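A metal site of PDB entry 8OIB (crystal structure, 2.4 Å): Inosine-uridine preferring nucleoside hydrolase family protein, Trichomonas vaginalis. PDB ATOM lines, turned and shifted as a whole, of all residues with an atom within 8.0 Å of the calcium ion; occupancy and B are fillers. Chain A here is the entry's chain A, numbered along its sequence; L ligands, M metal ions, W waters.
ND2 of Asn 39 touches the calcium ion, 3.96 Å away. Along chain A the residues within 4 Å of the calcium ion span positions 10 to 263.
The calcium ion is bound by O of Thr 142 (2.4 Å), O3 of the ligand (2.4 Å), water W1 (2.4 Å), OD1 of Asp 10 (2.4 Å), OD2 of Asp 15 (2.4 Å), OD2 of Asp 263 (2.4 Å), OD1 of Asp 15 (2.5 Å) and water W2 (2.5 Å). The calcium ion has eight donor atoms within binding distance.
Water W2 lies within hydrogen-bond range of the side-chain carboxylate (OD2) of Asp 10 (2.6 Å) and the side-chain amide oxygen (OD1) of Asn 184 (2.6 Å).
The backbone carbonyl oxygen (O) of Thr 142 lies close to the side-chain amide nitrogen (ND2) of Asn 184, at 3.3 Å. The backbone NH (N) of Thr 142 is in hydrogen-bond range of the backbone carbonyl oxygen (O) of Asp 8 (2.9 Å). ND2 of Asn 39 sits at hydrogen-bond distance from O of Asp 10, 2.8 Å away. ND2 of Asn 39 lies close to OD1 of Asp 15.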
ATOM      1  N   ASP A   8      25.025 -11.759   9.861  1.00  0.00           N
ATOM      2  CA  ASP A   8      24.807 -10.399  10.327  1.00  0.00           C
ATOM      3  C   ASP A   8      23.333 -10.285  10.717  1.00  0.00           C
ATOM      4  O   ASP A   8      22.469 -10.604   9.915  1.00  0.00           O
ATOM      5  CB  ASP A   8      25.220  -9.387   9.253  1.00  0.00           C
ATOM      6  CG  ASP A   8      25.521  -7.986   9.802  1.00  0.00           C
ATOM      7  OD1 ASP A   8      26.607  -7.808  10.396  1.00  0.00           O
ATOM      8  OD2 ASP A   8      24.659  -7.080   9.620  1.00  0.00           O
ATOM      9  N   CYS A   9      23.042  -9.876  11.960  1.00  0.00           N
ATOM     10  CA  CYS A   9      21.659  -9.971  12.432  1.00  0.00           C
ATOM     11  C   CYS A   9      21.426  -9.079  13.651  1.00  0.00           C
ATOM     12  O   CYS A   9      22.360  -8.501  14.192  1.00  0.00           O
ATOM     13  CB  CYS A   9      21.303 -11.415  12.745  1.00  0.00           C
ATOM     14  SG  CYS A   9      22.481 -12.208  13.884  1.00  0.00           S
ATOM     15  N   ASP A  10      20.141  -8.985  14.030  1.00  0.00           N
ATOM     16  CA  ASP A  10      19.658  -8.104  15.094  1.00  0.00           C
ATOM     17  C   ASP A  10      18.705  -8.864  16.011  1.00  0.00           C
ATOM     18  O   ASP A  10      17.561  -8.466  16.184  1.00  0.00           O
ATOM     19  CB  ASP A  10      18.979  -6.854  14.521  1.00  0.00           C
ATOM     20  CG  ASP A  10      17.809  -7.124  13.583  1.00  0.00           C
ATOM     21  OD1 ASP A  10      17.680  -8.265  13.107  1.00  0.00           O
ATOM     22  OD2 ASP A  10      17.001  -6.183  13.344  1.00  0.00           O
ATOM     23  N   PRO A  11      19.132  -9.973  16.665  1.00  0.00           N
ATOM     24  CA  PRO A  11      18.207 -10.813  17.434  1.00  0.00           C
ATOM     25  C   PRO A  11      17.448 -10.087  18.550  1.00  0.00           C
ATOM     26  O   PRO A  11      18.084  -9.431  19.362  1.00  0.00           O
ATOM     27  CB  PRO A  11      19.110 -11.893  18.056  1.00  0.00           C
ATOM     28  CG  PRO A  11      20.390 -11.866  17.254  1.00  0.00           C
ATOM     29  CD  PRO A  11      20.519 -10.461  16.715  1.00  0.00           C
ATOM     30  N   GLY A  12      16.099 -10.184  18.587  1.00  0.00           N
ATOM     31  CA  GLY A  12      15.233 -10.651  17.514  1.00  0.00           C
ATOM     32  C   GLY A  12      14.951 -12.156  17.579  1.00  0.00           C
ATOM     33  O   GLY A  12      15.891 -12.955  17.512  1.00  0.00           O
ATOM     34  N   HIS A  13      13.657 -12.525  17.631  1.00  0.00           N
ATOM     35  CA  HIS A  13      13.216 -13.913  17.750  1.00  0.00           C
ATOM     36  C   HIS A  13      13.471 -14.713  16.473  1.00  0.00           C
ATOM     37  O   HIS A  13      13.835 -15.874  16.524  1.00  0.00           O
ATOM     38  CB  HIS A  13      11.717 -13.985  18.089  1.00  0.00           C
ATOM     39  CG  HIS A  13      11.417 -13.376  19.410  1.00  0.00           C
ATOM     40  ND1 HIS A  13      11.324 -12.017  19.597  1.00  0.00           N
ATOM     41  CD2 HIS A  13      11.213 -13.923  20.606  1.00  0.00           C
ATOM     42  CE1 HIS A  13      11.084 -11.773  20.877  1.00  0.00           C
ATOM     43  NE2 HIS A  13      10.995 -12.924  21.510  1.00  0.00           N
ATOM     44  N   ASP A  14      13.215 -14.075  15.333  1.00  0.00           N
ATOM     45  CA  ASP A  14      13.505 -14.655  14.034  1.00  0.00           C
ATOM     46  C   ASP A  14      15.003 -14.906  13.908  1.00  0.00           C
ATOM     47  O   ASP A  14      15.402 -15.924  13.338  1.00  0.00           O
ATOM     48  CB  ASP A  14      13.167 -13.715  12.889  1.00  0.00           C
ATOM     49  CG  ASP A  14      11.754 -13.199  12.909  1.00  0.00           C
ATOM     50  OD1 ASP A  14      10.812 -14.033  12.837  1.00  0.00           O
ATOM     51  OD2 ASP A  14      11.625 -11.960  12.998  1.00  0.00           O
ATOM     52  N   ASP A  15      15.809 -13.917  14.343  1.00  0.00           N
ATOM     53  CA  ASP A  15      17.248 -13.963  14.143  1.00  0.00           C
ATOM     54  C   ASP A  15      17.805 -15.155  14.957  1.00  0.00           C
ATOM     55  O   ASP A  15      18.666 -15.903  14.483  1.00  0.00           O
ATOM     56  CB  ASP A  15      17.894 -12.599  14.446  1.00  0.00           C
ATOM     57  CG  ASP A  15      17.324 -11.380  13.723  1.00  0.00           C
ATOM     58  OD1 ASP A  15      16.230 -10.907  14.106  1.00  0.00           O
ATOM     59  OD2 ASP A  15      17.966 -10.877  12.775  1.00  0.00           O
ATOM     60  N   LEU A  16      17.263 -15.328  16.168  1.00  0.00           N
ATOM     61  CA  LEU A  16      17.599 -16.455  17.024  1.00  0.00           C
ATOM     62  C   LEU A  16      17.344 -17.789  16.309  1.00  0.00           C
ATOM     63  O   LEU A  16      18.192 -18.672  16.317  1.00  0.00           O
ATOM     64  CB  LEU A  16      16.803 -16.329  18.320  1.00  0.00           C
ATOM     65  CG  LEU A  16      16.745 -17.571  19.204  1.00  0.00           C
ATOM     66  CD1 LEU A  16      16.724 -17.160  20.673  1.00  0.00           C
ATOM     67  CD2 LEU A  16      15.517 -18.427  18.891  1.00  0.00           C
ATOM     68  N   MET A  18      17.264 -18.223  13.169  1.00  0.00           N
ATOM     69  CA  MET A  18      18.162 -18.292  12.019  1.00  0.00           C
ATOM     70  C   MET A  18      19.561 -18.736  12.467  1.00  0.00           C
ATOM     71  O   MET A  18      20.240 -19.456  11.756  1.00  0.00           O
ATOM     72  CB  MET A  18      18.260 -16.936  11.309  1.00  0.00           C
ATOM     73  CG  MET A  18      19.128 -16.958  10.060  1.00  0.00           C
ATOM     74  SD  MET A  18      20.871 -16.547  10.406  1.00  0.00           S
ATOM     75  CE  MET A  18      20.694 -14.932  11.183  1.00  0.00           C
ATOM     76  N   THR A  36      23.895  -5.948  14.696  1.00  0.00           N
ATOM     77  CA  THR A  36      23.628  -4.613  14.188  1.00  0.00           C
ATOM     78  C   THR A  36      22.486  -4.008  15.000  1.00  0.00           C
ATOM     79  O   THR A  36      21.805  -4.683  15.781  1.00  0.00           O
ATOM     80  CB  THR A  36      23.371  -4.663  12.687  1.00  0.00           C
ATOM     81  OG1 THR A  36      23.298  -3.322  12.187  1.00  0.00           O
ATOM     82  CG2 THR A  36      22.112  -5.417  12.306  1.00  0.00           C
ATOM     83  N   HIS A  37      22.323  -2.692  14.847  1.00  0.00           N
ATOM     84  CA  HIS A  37      21.161  -2.002  15.380  1.00  0.00           C
ATOM     85  C   HIS A  37      19.935  -2.526  14.640  1.00  0.00           C
ATOM     86  O   HIS A  37      20.032  -3.019  13.512  1.00  0.00           O
ATOM     87  CB  HIS A  37      21.308  -0.489  15.178  1.00  0.00           C
ATOM     88  CG  HIS A  37      21.416  -0.111  13.741  1.00  0.00           C
ATOM     89  ND1 HIS A  37      20.322   0.288  13.019  1.00  0.00           N
ATOM     90  CD2 HIS A  37      22.433  -0.125  12.882  1.00  0.00           C
ATOM     91  CE1 HIS A  37      20.698   0.535  11.768  1.00  0.00           C
ATOM     92  NE2 HIS A  37      21.989   0.284  11.663  1.00  0.00           N
ATOM     93  N   GLY A  38      18.773  -2.411  15.271  1.00  0.00           N
ATOM     94  CA  GLY A  38      17.525  -2.624  14.566  1.00  0.00           C
ATOM     95  C   GLY A  38      16.389  -2.811  15.540  1.00  0.00           C
ATOM     96  O   GLY A  38      15.914  -1.839  16.127  1.00  0.00           O
ATOM     97  N   ASN A  39      15.989  -4.083  15.700  1.00  0.00           N
ATOM     98  CA  ASN A  39      15.035  -4.482  16.708  1.00  0.00           C
ATOM     99  C   ASN A  39      15.347  -3.736  18.004  1.00  0.00           C
ATOM    100  O   ASN A  39      14.494  -3.025  18.539  1.00  0.00           O
ATOM    101  CB  ASN A  39      15.037  -6.012  16.837  1.00  0.00           C
ATOM    102  CG  ASN A  39      14.573  -6.700  15.569  1.00  0.00           C
ATOM    103  OD1 ASN A  39      13.908  -6.101  14.732  1.00  0.00           O
ATOM    104  ND2 ASN A  39      14.888  -7.973  15.418  1.00  0.00           N
ATOM    105  N   HIS A  83       9.380  -7.419  19.580  1.00  0.00           N
ATOM    106  CA  HIS A  83      10.467  -8.177  20.183  1.00  0.00           C
ATOM    107  C   HIS A  83      10.649  -7.933  21.693  1.00  0.00           C
ATOM    108  O   HIS A  83      11.370  -8.681  22.355  1.00  0.00           O
ATOM    109  CB  HIS A  83      11.760  -7.951  19.377  1.00  0.00           C
ATOM    110  CG  HIS A  83      11.658  -8.478  17.982  1.00  0.00           C
ATOM    111  ND1 HIS A  83      11.697  -9.813  17.689  1.00  0.00           N
ATOM    112  CD2 HIS A  83      11.542  -7.842  16.801  1.00  0.00           C
ATOM    113  CE1 HIS A  83      11.599  -9.993  16.386  1.00  0.00           C
ATOM    114  NE2 HIS A  83      11.497  -8.810  15.824  1.00  0.00           N
ATOM    115  N   SER A 141      22.466 -12.008   5.962  1.00  0.00           N
ATOM    116  CA  SER A 141      22.124 -10.755   6.599  1.00  0.00           C
ATOM    117  C   SER A 141      20.625 -10.759   6.873  1.00  0.00           C
ATOM    118  O   SER A 141      19.844 -11.009   5.954  1.00  0.00           O
ATOM    119  CB  SER A 141      22.545  -9.598   5.740  1.00  0.00           C
ATOM    120  OG  SER A 141      22.190  -8.361   6.341  1.00  0.00           O
ATOM    121  N   THR A 142      20.221 -10.536   8.126  1.00  0.00           N
ATOM    122  CA  THR A 142      18.813 -10.555   8.472  1.00  0.00           C
ATOM    123  C   THR A 142      18.456  -9.390   9.400  1.00  0.00           C
ATOM    124  O   THR A 142      17.425  -9.442  10.086  1.00  0.00           O
ATOM    125  CB  THR A 142      18.425 -11.907   9.063  1.00  0.00           C
ATOM    126  OG1 THR A 142      19.070 -12.057  10.326  1.00  0.00           O
ATOM    127  CG2 THR A 142      18.791 -13.060   8.153  1.00  0.00           C
ATOM    128  N   GLY A 143      19.295  -8.341   9.419  1.00  0.00           N
ATOM    129  CA  GLY A 143      18.975  -7.079  10.071  1.00  0.00           C
ATOM    130  C   GLY A 143      19.222  -5.899   9.136  1.00  0.00           C
ATOM    131  O   GLY A 143      19.169  -6.061   7.925  1.00  0.00           O
ATOM    132  N   SER A 144      19.530  -4.720   9.698  1.00  0.00           N
ATOM    133  CA  SER A 144      19.990  -3.605   8.885  1.00  0.00           C
ATOM    134  C   SER A 144      21.326  -3.982   8.276  1.00  0.00           C
ATOM    135  O   SER A 144      22.062  -4.746   8.874  1.00  0.00           O
ATOM    136  CB  SER A 144      20.128  -2.333   9.672  1.00  0.00           C
ATOM    137  OG  SER A 144      21.303  -2.383  10.466  1.00  0.00           O
ATOM    138  N   MET A 167      17.428 -11.572   4.339  1.00  0.00           N
ATOM    139  CA  MET A 167      16.021 -11.345   4.594  1.00  0.00           C
ATOM    140  C   MET A 167      15.807  -9.842   4.598  1.00  0.00           C
ATOM    141  O   MET A 167      16.291  -9.140   5.496  1.00  0.00           O
ATOM    142  CB  MET A 167      15.620 -11.982   5.925  1.00  0.00           C
ATOM    143  CG  MET A 167      14.124 -12.017   6.186  1.00  0.00           C
ATOM    144  SD  MET A 167      13.438 -10.391   6.605  1.00  0.00           S
ATOM    145  CE  MET A 167      12.077 -10.237   5.460  1.00  0.00           C
ATOM    146  N   GLU A 182       9.845  -2.655   4.121  1.00  0.00           N
ATOM    147  CA  GLU A 182      10.099  -3.668   5.117  1.00  0.00           C
ATOM    148  C   GLU A 182      11.132  -3.108   6.108  1.00  0.00           C
ATOM    149  O   GLU A 182      12.001  -2.339   5.715  1.00  0.00           O
ATOM    150  CB  GLU A 182      10.512  -4.945   4.380  1.00  0.00           C
ATOM    151  CG  GLU A 182      10.821  -6.114   5.286  1.00  0.00           C
ATOM    152  CD  GLU A 182      12.237  -6.143   5.844  1.00  0.00           C
ATOM    153  OE1 GLU A 182      13.183  -5.808   5.052  1.00  0.00           O
ATOM    154  OE2 GLU A 182      12.403  -6.505   7.054  1.00  0.00           O
ATOM    155  N   PHE A 183      11.030  -3.517   7.376  1.00  0.00           N
ATOM    156  CA  PHE A 183      11.833  -2.987   8.464  1.00  0.00           C
ATOM    157  C   PHE A 183      13.322  -2.886   8.147  1.00  0.00           C
ATOM    158  O   PHE A 183      13.923  -1.822   8.299  1.00  0.00           O
ATOM    159  CB  PHE A 183      11.651  -3.875   9.706  1.00  0.00           C
ATOM    160  CG  PHE A 183      12.338  -3.349  10.921  1.00  0.00           C
ATOM    161  CD1 PHE A 183      11.931  -2.161  11.495  1.00  0.00           C
ATOM    162  CD2 PHE A 183      13.432  -4.006  11.456  1.00  0.00           C
ATOM    163  CE1 PHE A 183      12.573  -1.639  12.608  1.00  0.00           C
ATOM    164  CE2 PHE A 183      14.073  -3.498  12.579  1.00  0.00           C
ATOM    165  CZ  PHE A 183      13.633  -2.321  13.154  1.00  0.00           C
ATOM    166  N   ASN A 184      13.942  -4.002   7.722  1.00  0.00           N
ATOM    167  CA  ASN A 184      15.384  -4.090   7.543  1.00  0.00           C
ATOM    168  C   ASN A 184      15.924  -3.089   6.528  1.00  0.00           C
ATOM    169  O   ASN A 184      17.053  -2.606   6.669  1.00  0.00           O
ATOM    170  CB  ASN A 184      15.829  -5.490   7.114  1.00  0.00           C
ATOM    171  CG  ASN A 184      15.706  -6.490   8.237  1.00  0.00           C
ATOM    172  OD1 ASN A 184      15.627  -6.120   9.410  1.00  0.00           O
ATOM    173  ND2 ASN A 184      15.691  -7.760   7.880  1.00  0.00           N
ATOM    174  N   ILE A 187      15.234   0.930   7.883  1.00  0.00           N
ATOM    175  CA  ILE A 187      16.075   1.469   8.938  1.00  0.00           C
ATOM    176  C   ILE A 187      17.424   1.936   8.403  1.00  0.00           C
ATOM    177  O   ILE A 187      18.042   2.779   9.058  1.00  0.00           O
ATOM    178  CB  ILE A 187      16.247   0.524  10.141  1.00  0.00           C
ATOM    179  CG1 ILE A 187      16.854  -0.811   9.742  1.00  0.00           C
ATOM    180  CG2 ILE A 187      14.935   0.366  10.870  1.00  0.00           C
ATOM    181  CD1 ILE A 187      16.854  -1.816  10.848  1.00  0.00           C
ATOM    182  N   HIS A 262      10.754 -15.232   9.679  1.00  0.00           N
ATOM    183  CA  HIS A 262      11.337 -14.551   8.544  1.00  0.00           C
ATOM    184  C   HIS A 262      12.768 -15.019   8.276  1.00  0.00           C
ATOM    185  O   HIS A 262      13.076 -15.592   7.218  1.00  0.00           O
ATOM    186  CB  HIS A 262      11.358 -13.037   8.777  1.00  0.00           C
ATOM    187  CG  HIS A 262      10.031 -12.382   8.920  1.00  0.00           C
ATOM    188  ND1 HIS A 262       9.207 -12.115   7.854  1.00  0.00           N
ATOM    189  CD2 HIS A 262       9.394 -11.880  10.005  1.00  0.00           C
ATOM    190  CE1 HIS A 262       8.110 -11.503   8.288  1.00  0.00           C
ATOM    191  NE2 HIS A 262       8.218 -11.350   9.594  1.00  0.00           N
ATOM    192  N   ASP A 263      13.642 -14.769   9.257  1.00  0.00           N
ATOM    193  CA  ASP A 263      15.081 -14.744   9.018  1.00  0.00           C
ATOM    194  C   ASP A 263      15.646 -16.114   8.635  1.00  0.00           C
ATOM    195  O   ASP A 263      16.508 -16.190   7.761  1.00  0.00           O
ATOM    196  CB  ASP A 263      15.779 -14.090  10.208  1.00  0.00           C
ATOM    197  CG  ASP A 263      15.393 -12.620  10.384  1.00  0.00           C
ATOM    198  OD1 ASP A 263      14.624 -12.109   9.552  1.00  0.00           O
ATOM    199  OD2 ASP A 263      15.872 -11.989  11.330  1.00  0.00           O
HETATM  200  C1  LIG L   1      10.669  -8.261   9.683  1.00  0.00           C
HETATM  201  O1  LIG L   1      10.871  -7.326   8.629  1.00  0.00           O
HETATM  202  C2  LIG L   1      11.932  -8.521  10.473  1.00  0.00           C
HETATM  203  O2  LIG L   1      11.703  -9.550  11.438  1.00  0.00           O
HETATM  204  C3  LIG L   1      13.119  -8.899   9.610  1.00  0.00           C
HETATM  205  O3  LIG L   1      14.234  -9.337  10.389  1.00  0.00           O
HETATM  206 CA    CA M   1      16.008  -9.642  12.005  1.00  0.00          CA
HETATM  207  O   HOH W   1      13.746 -10.030  12.801  1.00  0.00           O
HETATM  208  O   HOH W   2      15.397  -7.272  11.684  1.00  0.00           O
